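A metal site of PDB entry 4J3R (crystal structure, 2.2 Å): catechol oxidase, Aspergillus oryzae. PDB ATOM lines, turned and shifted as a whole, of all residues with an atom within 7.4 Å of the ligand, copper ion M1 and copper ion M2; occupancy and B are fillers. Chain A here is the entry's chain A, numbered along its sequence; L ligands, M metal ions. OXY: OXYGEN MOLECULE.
The side-chain hydroxyl (OG) of Ser 302 sits at hydrogen-bond distance from an oxygen (O1) of the ligand (3.3 Å).
A ring nitrogen (ND1) of His 119 sits at hydrogen-bond distance from the backbone carbonyl oxygen of Phe 115 (2.7 Å). The backbone carbonyl oxygen (O) of His 102 lies within hydrogen-bond range of the side-chain hydroxyl (OG1) of Thr 106. A ring nitrogen (NE2) of His 311 lies within hydrogen-bond range of the backbone carbonyl oxygen of His 284 (3.1 Å). A ring nitrogen (ND1) of His 110 is in hydrogen-bond range of the backbone carbonyl oxygen (O) of Thr 106. ND1 of His 102 sits at hydrogen-bond distance from O of Tyr 300 (2.8 Å).
Residues that only touch the ligand: Phe 308 (3.7 Å). Hydrophobic or aromatic side chains that line the ligand: His 102, His 110, His 119, His 284, His 288, Phe 308 and His 312. Within 4 Å of the ligand: His 102, His 110, His 119, His 284, His 288, Ser 302, Phe 308 and His 312. Along chain A the residues within 4 Å of the ligand span positions 102 to 312. The nearest printed residue that does not touch the ligand is Val 299 (4.1 Å).
Of the 23 residues printed, 3 come within 4 Å of copper ion M2. Along chain A the residues within 4 Å of copper ion M2 span positions 102 to 119.
Copper ion M1 is bound by a ring nitrogen (NE2) of His 312 (1.9 Å), a ring nitrogen (NE2) of His 288 (2.0 Å), a ring nitrogen (NE2) of His 284 (2.0 Å) and an oxygen (O2) of the ligand (2.3 Å). Copper ion M1 has four donor atoms within binding distance.
Copper ion M2 is bound by a ring nitrogen (NE2) of His 102 (1.9 Å), a ring nitrogen (NE2) of His 119 (2.0 Å), an oxygen (O2) of the ligand (2.1 Å) and a ring nitrogen (NE2) of His 110 (2.1 Å).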
ATOM      1  N   HIS A 102       8.788  13.243  10.914  1.00  0.00           N
ATOM      2  CA  HIS A 102       7.909  12.587  11.875  1.00  0.00           C
ATOM      3  C   HIS A 102       8.679  11.571  12.713  1.00  0.00           C
ATOM      4  O   HIS A 102       8.492  11.473  13.935  1.00  0.00           O
ATOM      5  CB  HIS A 102       6.740  11.910  11.169  1.00  0.00           C
ATOM      6  CG  HIS A 102       5.666  11.464  12.105  1.00  0.00           C
ATOM      7  ND1 HIS A 102       5.653  10.212  12.691  1.00  0.00           N
ATOM      8  CD2 HIS A 102       4.576  12.107  12.578  1.00  0.00           C
ATOM      9  CE1 HIS A 102       4.593  10.091  13.460  1.00  0.00           C
ATOM     10  NE2 HIS A 102       3.927  11.233  13.415  1.00  0.00           N
ATOM     11  N   GLN A 105      10.951  13.281  15.273  1.00  0.00           N
ATOM     12  CA  GLN A 105      10.318  14.024  16.360  1.00  0.00           C
ATOM     13  C   GLN A 105       9.238  13.236  17.114  1.00  0.00           C
ATOM     14  O   GLN A 105       8.494  13.827  17.903  1.00  0.00           O
ATOM     15  CB  GLN A 105       9.697  15.317  15.840  1.00  0.00           C
ATOM     16  CG  GLN A 105      10.658  16.257  15.118  1.00  0.00           C
ATOM     17  CD  GLN A 105      10.048  17.656  14.908  1.00  0.00           C
ATOM     18  OE1 GLN A 105       9.535  18.264  15.851  1.00  0.00           O
ATOM     19  NE2 GLN A 105      10.095  18.153  13.684  1.00  0.00           N
ATOM     20  N   THR A 106       9.158  11.930  16.877  1.00  0.00           N
ATOM     21  CA  THR A 106       8.078  11.112  17.427  1.00  0.00           C
ATOM     22  C   THR A 106       7.954  11.198  18.946  1.00  0.00           C
ATOM     23  O   THR A 106       6.858  11.230  19.482  1.00  0.00           O
ATOM     24  CB  THR A 106       8.226   9.626  16.982  1.00  0.00           C
ATOM     25  OG1 THR A 106       7.712   9.482  15.655  1.00  0.00           O
ATOM     26  CG2 THR A 106       7.478   8.691  17.903  1.00  0.00           C
ATOM     27  N   ILE A 109       6.080  14.569  20.004  1.00  0.00           N
ATOM     28  CA  ILE A 109       4.844  15.002  19.338  1.00  0.00           C
ATOM     29  C   ILE A 109       3.649  14.085  19.589  1.00  0.00           C
ATOM     30  O   ILE A 109       2.578  14.298  19.048  1.00  0.00           O
ATOM     31  CB  ILE A 109       5.033  15.165  17.817  1.00  0.00           C
ATOM     32  CG1 ILE A 109       5.367  13.808  17.174  1.00  0.00           C
ATOM     33  CG2 ILE A 109       6.088  16.231  17.511  1.00  0.00           C
ATOM     34  CD1 ILE A 109       5.546  13.901  15.667  1.00  0.00           C
ATOM     35  N   HIS A 110       3.836  13.060  20.421  1.00  0.00           N
ATOM     36  CA  HIS A 110       2.740  12.191  20.802  1.00  0.00           C
ATOM     37  C   HIS A 110       2.669  12.180  22.313  1.00  0.00           C
ATOM     38  O   HIS A 110       3.703  12.206  22.977  1.00  0.00           O
ATOM     39  CB  HIS A 110       2.927  10.775  20.233  1.00  0.00           C
ATOM     40  CG  HIS A 110       2.972  10.728  18.740  1.00  0.00           C
ATOM     41  ND1 HIS A 110       4.150  10.646  18.024  1.00  0.00           N
ATOM     42  CD2 HIS A 110       1.980  10.749  17.819  1.00  0.00           C
ATOM     43  CE1 HIS A 110       3.882  10.621  16.732  1.00  0.00           C
ATOM     44  NE2 HIS A 110       2.577  10.682  16.575  1.00  0.00           N
ATOM     45  N   PHE A 115       0.884  17.653  20.599  1.00  0.00           N
ATOM     46  CA  PHE A 115       0.377  16.594  19.700  1.00  0.00           C
ATOM     47  C   PHE A 115      -0.657  17.055  18.651  1.00  0.00           C
ATOM     48  O   PHE A 115      -0.436  16.893  17.441  1.00  0.00           O
ATOM     49  CB  PHE A 115      -0.187  15.430  20.517  1.00  0.00           C
ATOM     50  CG  PHE A 115      -1.025  14.479  19.717  1.00  0.00           C
ATOM     51  CD1 PHE A 115      -0.443  13.615  18.799  1.00  0.00           C
ATOM     52  CD2 PHE A 115      -2.394  14.434  19.895  1.00  0.00           C
ATOM     53  CE1 PHE A 115      -1.225  12.741  18.056  1.00  0.00           C
ATOM     54  CE2 PHE A 115      -3.187  13.565  19.165  1.00  0.00           C
ATOM     55  CZ  PHE A 115      -2.600  12.714  18.245  1.00  0.00           C
ATOM     56  N   TRP A 118       0.738  20.167  16.442  1.00  0.00           N
ATOM     57  CA  TRP A 118       1.825  19.746  15.573  1.00  0.00           C
ATOM     58  C   TRP A 118       1.279  18.999  14.355  1.00  0.00           C
ATOM     59  O   TRP A 118       1.650  19.296  13.209  1.00  0.00           O
ATOM     60  CB  TRP A 118       2.840  18.890  16.332  1.00  0.00           C
ATOM     61  CG  TRP A 118       4.071  18.594  15.560  1.00  0.00           C
ATOM     62  CD1 TRP A 118       5.280  19.241  15.654  1.00  0.00           C
ATOM     63  CD2 TRP A 118       4.238  17.569  14.574  1.00  0.00           C
ATOM     64  NE1 TRP A 118       6.178  18.669  14.790  1.00  0.00           N
ATOM     65  CE2 TRP A 118       5.569  17.649  14.106  1.00  0.00           C
ATOM     66  CE3 TRP A 118       3.382  16.594  14.035  1.00  0.00           C
ATOM     67  CZ2 TRP A 118       6.068  16.785  13.124  1.00  0.00           C
ATOM     68  CZ3 TRP A 118       3.884  15.730  13.062  1.00  0.00           C
ATOM     69  CH2 TRP A 118       5.221  15.833  12.623  1.00  0.00           C
ATOM     70  N   HIS A 119       0.384  18.054  14.581  1.00  0.00           N
ATOM     71  CA  HIS A 119      -0.156  17.292  13.454  1.00  0.00           C
ATOM     72  C   HIS A 119      -1.024  18.179  12.571  1.00  0.00           C
ATOM     73  O   HIS A 119      -1.045  18.020  11.341  1.00  0.00           O
ATOM     74  CB  HIS A 119      -0.904  16.045  13.945  1.00  0.00           C
ATOM     75  CG  HIS A 119       0.017  14.975  14.455  1.00  0.00           C
ATOM     76  ND1 HIS A 119       0.589  15.030  15.710  1.00  0.00           N
ATOM     77  CD2 HIS A 119       0.484  13.850  13.877  1.00  0.00           C
ATOM     78  CE1 HIS A 119       1.360  13.970  15.884  1.00  0.00           C
ATOM     79  NE2 HIS A 119       1.316  13.242  14.780  1.00  0.00           N
ATOM     80  N   PHE A 122       1.559  19.803  10.550  1.00  0.00           N
ATOM     81  CA  PHE A 122       2.169  18.784   9.682  1.00  0.00           C
ATOM     82  C   PHE A 122       1.350  18.610   8.391  1.00  0.00           C
ATOM     83  O   PHE A 122       1.862  18.793   7.280  1.00  0.00           O
ATOM     84  CB  PHE A 122       2.279  17.454  10.448  1.00  0.00           C
ATOM     85  CG  PHE A 122       3.191  16.434   9.811  1.00  0.00           C
ATOM     86  CD1 PHE A 122       4.425  16.792   9.294  1.00  0.00           C
ATOM     87  CD2 PHE A 122       2.827  15.096   9.791  1.00  0.00           C
ATOM     88  CE1 PHE A 122       5.270  15.826   8.721  1.00  0.00           C
ATOM     89  CE2 PHE A 122       3.666  14.126   9.230  1.00  0.00           C
ATOM     90  CZ  PHE A 122       4.879  14.498   8.696  1.00  0.00           C
ATOM     91  N   GLN A 273      -6.067   9.499  22.047  1.00  0.00           N
ATOM     92  CA  GLN A 273      -4.856   8.719  21.818  1.00  0.00           C
ATOM     93  C   GLN A 273      -4.896   7.359  22.506  1.00  0.00           C
ATOM     94  O   GLN A 273      -4.122   6.467  22.161  1.00  0.00           O
ATOM     95  CB  GLN A 273      -3.615   9.488  22.290  1.00  0.00           C
ATOM     96  CG  GLN A 273      -3.160  10.537  21.306  1.00  0.00           C
ATOM     97  CD  GLN A 273      -2.157  11.497  21.915  1.00  0.00           C
ATOM     98  OE1 GLN A 273      -0.958  11.393  21.677  1.00  0.00           O
ATOM     99  NE2 GLN A 273      -2.663  12.448  22.702  1.00  0.00           N
ATOM    100  N   HIS A 284      -7.474   7.493  17.535  1.00  0.00           N
ATOM    101  CA  HIS A 284      -6.205   7.756  16.880  1.00  0.00           C
ATOM    102  C   HIS A 284      -5.428   6.461  16.660  1.00  0.00           C
ATOM    103  O   HIS A 284      -4.911   6.237  15.582  1.00  0.00           O
ATOM    104  CB  HIS A 284      -5.341   8.741  17.663  1.00  0.00           C
ATOM    105  CG  HIS A 284      -4.001   8.967  17.045  1.00  0.00           C
ATOM    106  ND1 HIS A 284      -2.829   8.565  17.642  1.00  0.00           N
ATOM    107  CD2 HIS A 284      -3.650   9.532  15.864  1.00  0.00           C
ATOM    108  CE1 HIS A 284      -1.813   8.875  16.866  1.00  0.00           C
ATOM    109  NE2 HIS A 284      -2.280   9.451  15.772  1.00  0.00           N
ATOM    110  N   GLY A 285      -5.359   5.622  17.697  1.00  0.00           N
ATOM    111  CA  GLY A 285      -4.682   4.339  17.611  1.00  0.00           C
ATOM    112  C   GLY A 285      -5.425   3.395  16.698  1.00  0.00           C
ATOM    113  O   GLY A 285      -4.826   2.743  15.841  1.00  0.00           O
ATOM    114  N   HIS A 288      -4.858   4.165  13.036  1.00  0.00           N
ATOM    115  CA  HIS A 288      -3.523   3.715  12.646  1.00  0.00           C
ATOM    116  C   HIS A 288      -3.437   2.203  12.513  1.00  0.00           C
ATOM    117  O   HIS A 288      -3.082   1.685  11.459  1.00  0.00           O
ATOM    118  CB  HIS A 288      -2.481   4.206  13.642  1.00  0.00           C
ATOM    119  CG  HIS A 288      -2.051   5.612  13.410  1.00  0.00           C
ATOM    120  ND1 HIS A 288      -1.405   6.022  12.262  1.00  0.00           N
ATOM    121  CD2 HIS A 288      -2.174   6.725  14.179  1.00  0.00           C
ATOM    122  CE1 HIS A 288      -1.142   7.311  12.336  1.00  0.00           C
ATOM    123  NE2 HIS A 288      -1.598   7.755  13.486  1.00  0.00           N
ATOM    124  N   ASP A 298       3.913   1.103  13.021  1.00  0.00           N
ATOM    125  CA  ASP A 298       5.110   1.740  13.527  1.00  0.00           C
ATOM    126  C   ASP A 298       4.770   3.189  13.892  1.00  0.00           C
ATOM    127  O   ASP A 298       4.578   4.028  13.005  1.00  0.00           O
ATOM    128  CB  ASP A 298       6.189   1.670  12.453  1.00  0.00           C
ATOM    129  CG  ASP A 298       7.560   2.122  12.948  1.00  0.00           C
ATOM    130  OD1 ASP A 298       7.647   3.184  13.601  1.00  0.00           O
ATOM    131  OD2 ASP A 298       8.558   1.426  12.650  1.00  0.00           O
ATOM    132  N   VAL A 299       4.695   3.488  15.179  1.00  0.00           N
ATOM    133  CA  VAL A 299       4.331   4.833  15.624  1.00  0.00           C
ATOM    134  C   VAL A 299       5.193   5.923  14.970  1.00  0.00           C
ATOM    135  O   VAL A 299       4.701   6.976  14.623  1.00  0.00           O
ATOM    136  CB  VAL A 299       4.377   4.972  17.156  1.00  0.00           C
ATOM    137  CG1 VAL A 299       4.022   6.391  17.546  1.00  0.00           C
ATOM    138  CG2 VAL A 299       3.383   4.011  17.794  1.00  0.00           C
ATOM    139  N   TYR A 300       6.477   5.647  14.749  1.00  0.00           N
ATOM    140  CA  TYR A 300       7.367   6.677  14.193  1.00  0.00           C
ATOM    141  C   TYR A 300       7.170   6.884  12.704  1.00  0.00           C
ATOM    142  O   TYR A 300       7.283   7.999  12.223  1.00  0.00           O
ATOM    143  CB  TYR A 300       8.825   6.277  14.379  1.00  0.00           C
ATOM    144  CG  TYR A 300       9.306   6.125  15.795  1.00  0.00           C
ATOM    145  CD1 TYR A 300      10.278   6.980  16.302  1.00  0.00           C
ATOM    146  CD2 TYR A 300       8.818   5.116  16.620  1.00  0.00           C
ATOM    147  CE1 TYR A 300      10.747   6.842  17.597  1.00  0.00           C
ATOM    148  CE2 TYR A 300       9.269   4.969  17.919  1.00  0.00           C
ATOM    149  CZ  TYR A 300      10.229   5.841  18.408  1.00  0.00           C
ATOM    150  OH  TYR A 300      10.697   5.694  19.683  1.00  0.00           O
ATOM    151  N   VAL A 301       6.921   5.798  11.984  1.00  0.00           N
ATOM    152  CA  VAL A 301       7.075   5.776  10.528  1.00  0.00           C
ATOM    153  C   VAL A 301       5.710   5.844   9.841  1.00  0.00           C
ATOM    154  O   VAL A 301       5.622   5.929   8.618  1.00  0.00           O
ATOM    155  CB  VAL A 301       7.875   4.494  10.098  1.00  0.00           C
ATOM    156  CG1 VAL A 301       8.287   4.545   8.634  1.00  0.00           C
ATOM    157  CG2 VAL A 301       9.100   4.374  10.950  1.00  0.00           C
ATOM    158  N   SER A 302       4.654   5.854  10.645  1.00  0.00           N
ATOM    159  CA  SER A 302       3.284   5.876  10.135  1.00  0.00           C
ATOM    160  C   SER A 302       2.949   6.835   8.968  1.00  0.00           C
ATOM    161  O   SER A 302       2.094   6.493   8.153  1.00  0.00           O
ATOM    162  CB  SER A 302       2.281   6.064  11.280  1.00  0.00           C
ATOM    163  OG  SER A 302       2.404   7.357  11.826  1.00  0.00           O
ATOM    164  N   PRO A 303       3.613   7.997   8.867  1.00  0.00           N
ATOM    165  CA  PRO A 303       3.256   8.803   7.690  1.00  0.00           C
ATOM    166  C   PRO A 303       3.724   8.200   6.368  1.00  0.00           C
ATOM    167  O   PRO A 303       3.381   8.720   5.310  1.00  0.00           O
ATOM    168  CB  PRO A 303       3.987  10.138   7.927  1.00  0.00           C
ATOM    169  CG  PRO A 303       4.237  10.166   9.387  1.00  0.00           C
ATOM    170  CD  PRO A 303       4.480   8.755   9.790  1.00  0.00           C
ATOM    171  N   PHE A 308      -2.159   7.947   6.065  1.00  0.00           N
ATOM    172  CA  PHE A 308      -1.850   8.801   7.209  1.00  0.00           C
ATOM    173  C   PHE A 308      -2.526  10.174   7.097  1.00  0.00           C
ATOM    174  O   PHE A 308      -3.129  10.642   8.053  1.00  0.00           O
ATOM    175  CB  PHE A 308      -0.341   8.989   7.334  1.00  0.00           C
ATOM    176  CG  PHE A 308       0.075   9.893   8.453  1.00  0.00           C
ATOM    177  CD1 PHE A 308       0.064  11.284   8.277  1.00  0.00           C
ATOM    178  CD2 PHE A 308       0.489   9.373   9.669  1.00  0.00           C
ATOM    179  CE1 PHE A 308       0.448  12.136   9.302  1.00  0.00           C
ATOM    180  CE2 PHE A 308       0.875  10.226  10.704  1.00  0.00           C
ATOM    181  CZ  PHE A 308       0.857  11.603  10.520  1.00  0.00           C
ATOM    182  N   HIS A 311      -6.296  10.062   7.577  1.00  0.00           N
ATOM    183  CA  HIS A 311      -6.541   9.749   8.993  1.00  0.00           C
ATOM    184  C   HIS A 311      -6.422  11.019   9.857  1.00  0.00           C
ATOM    185  O   HIS A 311      -7.302  11.329  10.664  1.00  0.00           O
ATOM    186  CB  HIS A 311      -5.545   8.694   9.465  1.00  0.00           C
ATOM    187  CG  HIS A 311      -5.654   8.351  10.923  1.00  0.00           C
ATOM    188  ND1 HIS A 311      -6.848   8.049  11.532  1.00  0.00           N
ATOM    189  CD2 HIS A 311      -4.706   8.253  11.887  1.00  0.00           C
ATOM    190  CE1 HIS A 311      -6.640   7.784  12.806  1.00  0.00           C
ATOM    191  NE2 HIS A 311      -5.350   7.897  13.053  1.00  0.00           N
ATOM    192  N   HIS A 312      -5.332  11.753   9.666  1.00  0.00           N
ATOM    193  CA  HIS A 312      -5.102  12.924  10.469  1.00  0.00           C
ATOM    194  C   HIS A 312      -5.950  14.110  10.022  1.00  0.00           C
ATOM    195  O   HIS A 312      -6.156  15.033  10.784  1.00  0.00           O
ATOM    196  CB  HIS A 312      -3.623  13.264  10.575  1.00  0.00           C
ATOM    197  CG  HIS A 312      -2.971  12.591  11.735  1.00  0.00           C
ATOM    198  ND1 HIS A 312      -2.954  13.142  13.003  1.00  0.00           N
ATOM    199  CD2 HIS A 312      -2.400  11.369  11.844  1.00  0.00           C
ATOM    200  CE1 HIS A 312      -2.366  12.297  13.834  1.00  0.00           C
ATOM    201  NE2 HIS A 312      -2.011  11.216  13.157  1.00  0.00           N
ATOM    202  N   ILE A 315      -8.595  13.296  12.327  1.00  0.00           N
ATOM    203  CA  ILE A 315      -8.177  13.659  13.678  1.00  0.00           C
ATOM    204  C   ILE A 315      -8.345  15.173  13.901  1.00  0.00           C
ATOM    205  O   ILE A 315      -8.894  15.605  14.918  1.00  0.00           O
ATOM    206  CB  ILE A 315      -6.722  13.240  13.957  1.00  0.00           C
ATOM    207  CG1 ILE A 315      -6.587  11.709  13.947  1.00  0.00           C
ATOM    208  CG2 ILE A 315      -6.240  13.798  15.298  1.00  0.00           C
ATOM    209  CD1 ILE A 315      -7.200  11.046  15.167  1.00  0.00           C
HETATM  210  O1  OXY L   1       1.268   9.237  14.225  1.00  0.00           O
HETATM  211  O2  OXY L   1       0.810  10.266  14.650  1.00  0.00           O
HETATM  212 CU    CU M   1      -1.330   9.643  14.001  1.00  0.00          CU
HETATM  213 CU    CU M   2       2.456  11.558  14.617  1.00  0.00          CU
